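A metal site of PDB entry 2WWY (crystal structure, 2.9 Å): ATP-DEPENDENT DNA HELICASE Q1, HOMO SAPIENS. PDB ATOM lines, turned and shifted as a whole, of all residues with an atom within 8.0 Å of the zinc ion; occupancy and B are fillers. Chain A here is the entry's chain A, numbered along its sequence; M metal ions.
SG of Cys 428 binds the zinc ion.
The zinc ion is bound by SG of Cys 431, 2.3 Å away.
SG of Cys 424 is bound to the zinc ion (2.3 Å).
The zinc ion is bound by the side-chain sulfur (SG) of Cys 406 (2.3 Å).
The zinc ion has four donor atoms within binding distance.
Four residues have an atom within 4 Å of the zinc ion: Cys 406, Cys 424, Cys 428 and Cys 431.
The nearest printed residue that does not touch the zinc ion is Arg 407 (4.1 Å).
The side-chain sulfur of Cys 428 sits close to the backbone NH of Arg 407 (3.4 Å).
The side-chain sulfur of Cys 432 sits at hydrogen-bond distance from the backbone carbonyl oxygen of Cys 428.
SG of Cys 424 sits close to N of Met 427 (3.6 Å).
SG of Cys 406 sits close to N of Arg 408 (3.8 Å).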
ATOM      1  N   TYR A 240      24.621 -15.343 -33.175  1.00  0.00           N
ATOM      2  CA  TYR A 240      23.283 -15.969 -33.308  1.00  0.00           C
ATOM      3  C   TYR A 240      23.351 -17.531 -33.357  1.00  0.00           C
ATOM      4  O   TYR A 240      24.031 -18.081 -34.217  1.00  0.00           O
ATOM      5  CB  TYR A 240      22.500 -15.396 -34.520  1.00  0.00           C
ATOM      6  CG  TYR A 240      21.173 -16.091 -34.831  1.00  0.00           C
ATOM      7  CD1 TYR A 240      19.974 -15.662 -34.255  1.00  0.00           C
ATOM      8  CD2 TYR A 240      21.121 -17.200 -35.679  1.00  0.00           C
ATOM      9  CE1 TYR A 240      18.753 -16.318 -34.515  1.00  0.00           C
ATOM     10  CE2 TYR A 240      19.921 -17.854 -35.947  1.00  0.00           C
ATOM     11  CZ  TYR A 240      18.745 -17.406 -35.370  1.00  0.00           C
ATOM     12  OH  TYR A 240      17.559 -18.062 -35.639  1.00  0.00           O
ATOM     13  N   TYR A 241      22.646 -18.223 -32.445  1.00  0.00           N
ATOM     14  CA  TYR A 241      22.785 -19.697 -32.284  1.00  0.00           C
ATOM     15  C   TYR A 241      21.596 -20.524 -32.814  1.00  0.00           C
ATOM     16  O   TYR A 241      20.467 -20.300 -32.407  1.00  0.00           O
ATOM     17  CB  TYR A 241      22.976 -20.072 -30.788  1.00  0.00           C
ATOM     18  CG  TYR A 241      24.297 -19.651 -30.156  1.00  0.00           C
ATOM     19  CD1 TYR A 241      25.492 -20.264 -30.524  1.00  0.00           C
ATOM     20  CD2 TYR A 241      24.348 -18.633 -29.195  1.00  0.00           C
ATOM     21  CE1 TYR A 241      26.691 -19.893 -29.964  1.00  0.00           C
ATOM     22  CE2 TYR A 241      25.550 -18.242 -28.609  1.00  0.00           C
ATOM     23  CZ  TYR A 241      26.734 -18.880 -29.013  1.00  0.00           C
ATOM     24  OH  TYR A 241      27.963 -18.545 -28.480  1.00  0.00           O
ATOM     25  N   SER A 404      12.687 -25.520 -26.755  1.00  0.00           N
ATOM     26  CA  SER A 404      12.047 -24.365 -26.144  1.00  0.00           C
ATOM     27  C   SER A 404      12.888 -23.458 -25.242  1.00  0.00           C
ATOM     28  O   SER A 404      12.527 -22.290 -25.080  1.00  0.00           O
ATOM     29  CB  SER A 404      10.737 -24.762 -25.446  1.00  0.00           C
ATOM     30  OG  SER A 404      10.967 -25.663 -24.392  1.00  0.00           O
ATOM     31  N   LYS A 405      13.987 -23.951 -24.667  1.00  0.00           N
ATOM     32  CA  LYS A 405      14.733 -23.087 -23.747  1.00  0.00           C
ATOM     33  C   LYS A 405      15.707 -22.263 -24.540  1.00  0.00           C
ATOM     34  O   LYS A 405      16.158 -22.704 -25.580  1.00  0.00           O
ATOM     35  CB  LYS A 405      15.444 -23.890 -22.666  1.00  0.00           C
ATOM     36  CG  LYS A 405      14.663 -25.130 -22.190  1.00  0.00           C
ATOM     37  CD  LYS A 405      13.493 -24.821 -21.184  1.00  0.00           C
ATOM     38  CE  LYS A 405      12.453 -25.996 -21.084  1.00  0.00           C
ATOM     39  NZ  LYS A 405      13.050 -27.412 -21.305  1.00  0.00           N
ATOM     40  N   CYS A 406      16.002 -21.049 -24.070  1.00  0.00           N
ATOM     41  CA  CYS A 406      17.042 -20.185 -24.645  1.00  0.00           C
ATOM     42  C   CYS A 406      18.438 -20.884 -24.734  1.00  0.00           C
ATOM     43  O   CYS A 406      18.862 -21.539 -23.788  1.00  0.00           O
ATOM     44  CB  CYS A 406      17.179 -18.933 -23.788  1.00  0.00           C
ATOM     45  SG  CYS A 406      18.196 -17.672 -24.518  1.00  0.00           S
ATOM     46  N   ARG A 407      19.120 -20.769 -25.860  1.00  0.00           N
ATOM     47  CA  ARG A 407      20.435 -21.415 -25.969  1.00  0.00           C
ATOM     48  C   ARG A 407      21.447 -20.922 -24.915  1.00  0.00           C
ATOM     49  O   ARG A 407      22.233 -21.702 -24.387  1.00  0.00           O
ATOM     50  CB  ARG A 407      21.033 -21.261 -27.374  1.00  0.00           C
ATOM     51  CG  ARG A 407      20.176 -21.812 -28.483  1.00  0.00           C
ATOM     52  CD  ARG A 407      20.025 -23.297 -28.387  1.00  0.00           C
ATOM     53  NE  ARG A 407      19.183 -23.776 -29.467  1.00  0.00           N
ATOM     54  CZ  ARG A 407      18.750 -25.017 -29.584  1.00  0.00           C
ATOM     55  NH1 ARG A 407      19.077 -25.934 -28.675  1.00  0.00           N
ATOM     56  NH2 ARG A 407      17.961 -25.347 -30.613  1.00  0.00           N
ATOM     57  N   ARG A 408      21.412 -19.624 -24.620  1.00  0.00           N
ATOM     58  CA  ARG A 408      22.294 -19.048 -23.610  1.00  0.00           C
ATOM     59  C   ARG A 408      22.036 -19.621 -22.192  1.00  0.00           C
ATOM     60  O   ARG A 408      22.964 -19.801 -21.392  1.00  0.00           O
ATOM     61  CB  ARG A 408      22.176 -17.509 -23.635  1.00  0.00           C
ATOM     62  CG  ARG A 408      23.099 -16.859 -24.651  1.00  0.00           C
ATOM     63  CD  ARG A 408      22.769 -15.408 -24.987  1.00  0.00           C
ATOM     64  NE  ARG A 408      23.785 -14.834 -25.876  1.00  0.00           N
ATOM     65  CZ  ARG A 408      23.740 -14.843 -27.205  1.00  0.00           C
ATOM     66  NH1 ARG A 408      24.720 -14.306 -27.921  1.00  0.00           N
ATOM     67  NH2 ARG A 408      22.699 -15.390 -27.833  1.00  0.00           N
ATOM     68  N   VAL A 409      20.765 -19.891 -21.867  1.00  0.00           N
ATOM     69  CA  VAL A 409      20.415 -20.516 -20.593  1.00  0.00           C
ATOM     70  C   VAL A 409      21.003 -21.946 -20.472  1.00  0.00           C
ATOM     71  O   VAL A 409      21.544 -22.317 -19.446  1.00  0.00           O
ATOM     72  CB  VAL A 409      18.853 -20.490 -20.336  1.00  0.00           C
ATOM     73  CG1 VAL A 409      18.399 -21.623 -19.438  1.00  0.00           C
ATOM     74  CG2 VAL A 409      18.426 -19.173 -19.740  1.00  0.00           C
ATOM     75  N   TRP A 419      23.013 -16.662 -14.602  1.00  0.00           N
ATOM     76  CA  TRP A 419      22.289 -16.057 -15.712  1.00  0.00           C
ATOM     77  C   TRP A 419      20.942 -15.412 -15.325  1.00  0.00           C
ATOM     78  O   TRP A 419      20.147 -16.018 -14.607  1.00  0.00           O
ATOM     79  CB  TRP A 419      22.093 -17.075 -16.837  1.00  0.00           C
ATOM     80  CG  TRP A 419      21.876 -16.459 -18.179  1.00  0.00           C
ATOM     81  CD1 TRP A 419      20.753 -16.559 -18.960  1.00  0.00           C
ATOM     82  CD2 TRP A 419      22.783 -15.627 -18.904  1.00  0.00           C
ATOM     83  NE1 TRP A 419      20.918 -15.844 -20.122  1.00  0.00           N
ATOM     84  CE2 TRP A 419      22.166 -15.266 -20.115  1.00  0.00           C
ATOM     85  CE3 TRP A 419      24.078 -15.157 -18.651  1.00  0.00           C
ATOM     86  CZ2 TRP A 419      22.780 -14.456 -21.061  1.00  0.00           C
ATOM     87  CZ3 TRP A 419      24.693 -14.347 -19.597  1.00  0.00           C
ATOM     88  CH2 TRP A 419      24.039 -14.016 -20.784  1.00  0.00           C
ATOM     89  N   SER A 421      17.417 -14.317 -16.908  1.00  0.00           N
ATOM     90  CA  SER A 421      16.713 -14.998 -17.998  1.00  0.00           C
ATOM     91  C   SER A 421      16.499 -14.271 -19.339  1.00  0.00           C
ATOM     92  O   SER A 421      16.577 -14.901 -20.406  1.00  0.00           O
ATOM     93  CB  SER A 421      15.363 -15.547 -17.504  1.00  0.00           C
ATOM     94  N   GLU A 422      16.229 -12.971 -19.301  1.00  0.00           N
ATOM     95  CA  GLU A 422      15.814 -12.271 -20.518  1.00  0.00           C
ATOM     96  C   GLU A 422      16.896 -11.370 -21.154  1.00  0.00           C
ATOM     97  O   GLU A 422      16.558 -10.365 -21.789  1.00  0.00           O
ATOM     98  CB  GLU A 422      14.528 -11.477 -20.263  1.00  0.00           C
ATOM     99  N   ALA A 423      18.165 -11.743 -21.013  1.00  0.00           N
ATOM    100  CA  ALA A 423      19.268 -10.928 -21.527  1.00  0.00           C
ATOM    101  C   ALA A 423      19.645 -11.314 -22.949  1.00  0.00           C
ATOM    102  O   ALA A 423      20.548 -10.703 -23.525  1.00  0.00           O
ATOM    103  CB  ALA A 423      20.495 -11.024 -20.609  1.00  0.00           C
ATOM    104  N   CYS A 424      18.958 -12.314 -23.503  1.00  0.00           N
ATOM    105  CA  CYS A 424      19.229 -12.799 -24.881  1.00  0.00           C
ATOM    106  C   CYS A 424      18.879 -11.778 -25.967  1.00  0.00           C
ATOM    107  O   CYS A 424      19.692 -11.547 -26.884  1.00  0.00           O
ATOM    108  CB  CYS A 424      18.562 -14.154 -25.163  1.00  0.00           C
ATOM    109  SG  CYS A 424      18.985 -14.938 -26.765  1.00  0.00           S
ATOM    110  N   ASN A 425      17.690 -11.152 -25.870  1.00  0.00           N
ATOM    111  CA  ASN A 425      17.236 -10.125 -26.809  1.00  0.00           C
ATOM    112  C   ASN A 425      16.885 -10.641 -28.200  1.00  0.00           C
ATOM    113  O   ASN A 425      17.100  -9.962 -29.191  1.00  0.00           O
ATOM    114  CB  ASN A 425      18.292  -9.037 -26.985  1.00  0.00           C
ATOM    115  CG  ASN A 425      18.493  -8.207 -25.733  1.00  0.00           C
ATOM    116  OD1 ASN A 425      17.552  -7.971 -24.949  1.00  0.00           O
ATOM    117  ND2 ASN A 425      19.728  -7.727 -25.554  1.00  0.00           N
ATOM    118  N   LYS A 426      16.350 -11.862 -28.266  1.00  0.00           N
ATOM    119  CA  LYS A 426      16.051 -12.497 -29.545  1.00  0.00           C
ATOM    120  C   LYS A 426      17.264 -12.785 -30.470  1.00  0.00           C
ATOM    121  O   LYS A 426      17.205 -12.544 -31.687  1.00  0.00           O
ATOM    122  CB  LYS A 426      14.948 -11.715 -30.266  1.00  0.00           C
ATOM    123  CG  LYS A 426      13.650 -11.596 -29.433  1.00  0.00           C
ATOM    124  CD  LYS A 426      12.473 -11.030 -30.224  1.00  0.00           C
ATOM    125  N   MET A 427      18.320 -13.368 -29.884  1.00  0.00           N
ATOM    126  CA  MET A 427      19.525 -13.802 -30.606  1.00  0.00           C
ATOM    127  C   MET A 427      19.793 -15.318 -30.595  1.00  0.00           C
ATOM    128  O   MET A 427      20.930 -15.742 -30.787  1.00  0.00           O
ATOM    129  CB  MET A 427      20.753 -13.082 -30.075  1.00  0.00           C
ATOM    130  CG  MET A 427      20.798 -11.600 -30.385  1.00  0.00           C
ATOM    131  SD  MET A 427      21.056 -11.133 -32.127  1.00  0.00           S
ATOM    132  CE  MET A 427      22.698 -11.754 -32.497  1.00  0.00           C
ATOM    133  N   CYS A 428      18.772 -16.138 -30.355  1.00  0.00           N
ATOM    134  CA  CYS A 428      18.878 -17.579 -30.676  1.00  0.00           C
ATOM    135  C   CYS A 428      17.596 -18.068 -31.383  1.00  0.00           C
ATOM    136  O   CYS A 428      16.577 -17.367 -31.409  1.00  0.00           O
ATOM    137  CB  CYS A 428      19.174 -18.442 -29.421  1.00  0.00           C
ATOM    138  SG  CYS A 428      17.748 -18.701 -28.256  1.00  0.00           S
ATOM    139  N   ASP A 429      17.637 -19.281 -31.936  1.00  0.00           N
ATOM    140  CA  ASP A 429      16.495 -19.777 -32.664  1.00  0.00           C
ATOM    141  C   ASP A 429      15.268 -20.017 -31.761  1.00  0.00           C
ATOM    142  O   ASP A 429      14.160 -19.615 -32.112  1.00  0.00           O
ATOM    143  CB  ASP A 429      16.858 -21.009 -33.502  1.00  0.00           C
ATOM    144  CG  ASP A 429      17.254 -22.216 -32.661  1.00  0.00           C
ATOM    145  OD1 ASP A 429      17.309 -23.339 -33.240  1.00  0.00           O
ATOM    146  OD2 ASP A 429      17.534 -22.068 -31.440  1.00  0.00           O
ATOM    147  N   ASN A 430      15.454 -20.629 -30.599  1.00  0.00           N
ATOM    148  CA  ASN A 430      14.321 -20.914 -29.720  1.00  0.00           C
ATOM    149  C   ASN A 430      13.688 -19.643 -29.161  1.00  0.00           C
ATOM    150  O   ASN A 430      12.521 -19.662 -28.797  1.00  0.00           O
ATOM    151  CB  ASN A 430      14.715 -21.877 -28.581  1.00  0.00           C
ATOM    152  CG  ASN A 430      14.931 -23.329 -29.061  1.00  0.00           C
ATOM    153  OD1 ASN A 430      14.554 -23.692 -30.168  1.00  0.00           O
ATOM    154  ND2 ASN A 430      15.512 -24.163 -28.200  1.00  0.00           N
ATOM    155  N   CYS A 431      14.426 -18.538 -29.093  1.00  0.00           N
ATOM    156  CA  CYS A 431      13.875 -17.280 -28.573  1.00  0.00           C
ATOM    157  C   CYS A 431      13.075 -16.526 -29.646  1.00  0.00           C
ATOM    158  O   CYS A 431      12.355 -15.577 -29.344  1.00  0.00           O
ATOM    159  CB  CYS A 431      14.982 -16.368 -27.990  1.00  0.00           C
ATOM    160  SG  CYS A 431      15.523 -16.661 -26.251  1.00  0.00           S
ATOM    161  N   CYS A 432      13.209 -16.947 -30.917  1.00  0.00           N
ATOM    162  CA  CYS A 432      12.481 -16.320 -32.024  1.00  0.00           C
ATOM    163  C   CYS A 432      11.257 -17.103 -32.500  1.00  0.00           C
ATOM    164  O   CYS A 432      10.455 -16.569 -33.272  1.00  0.00           O
ATOM    165  CB  CYS A 432      13.399 -16.068 -33.210  1.00  0.00           C
ATOM    166  SG  CYS A 432      14.548 -14.722 -32.939  1.00  0.00           S
HETATM  167 ZN    ZN M   1      17.795 -16.953 -26.709  1.00  0.00          ZN
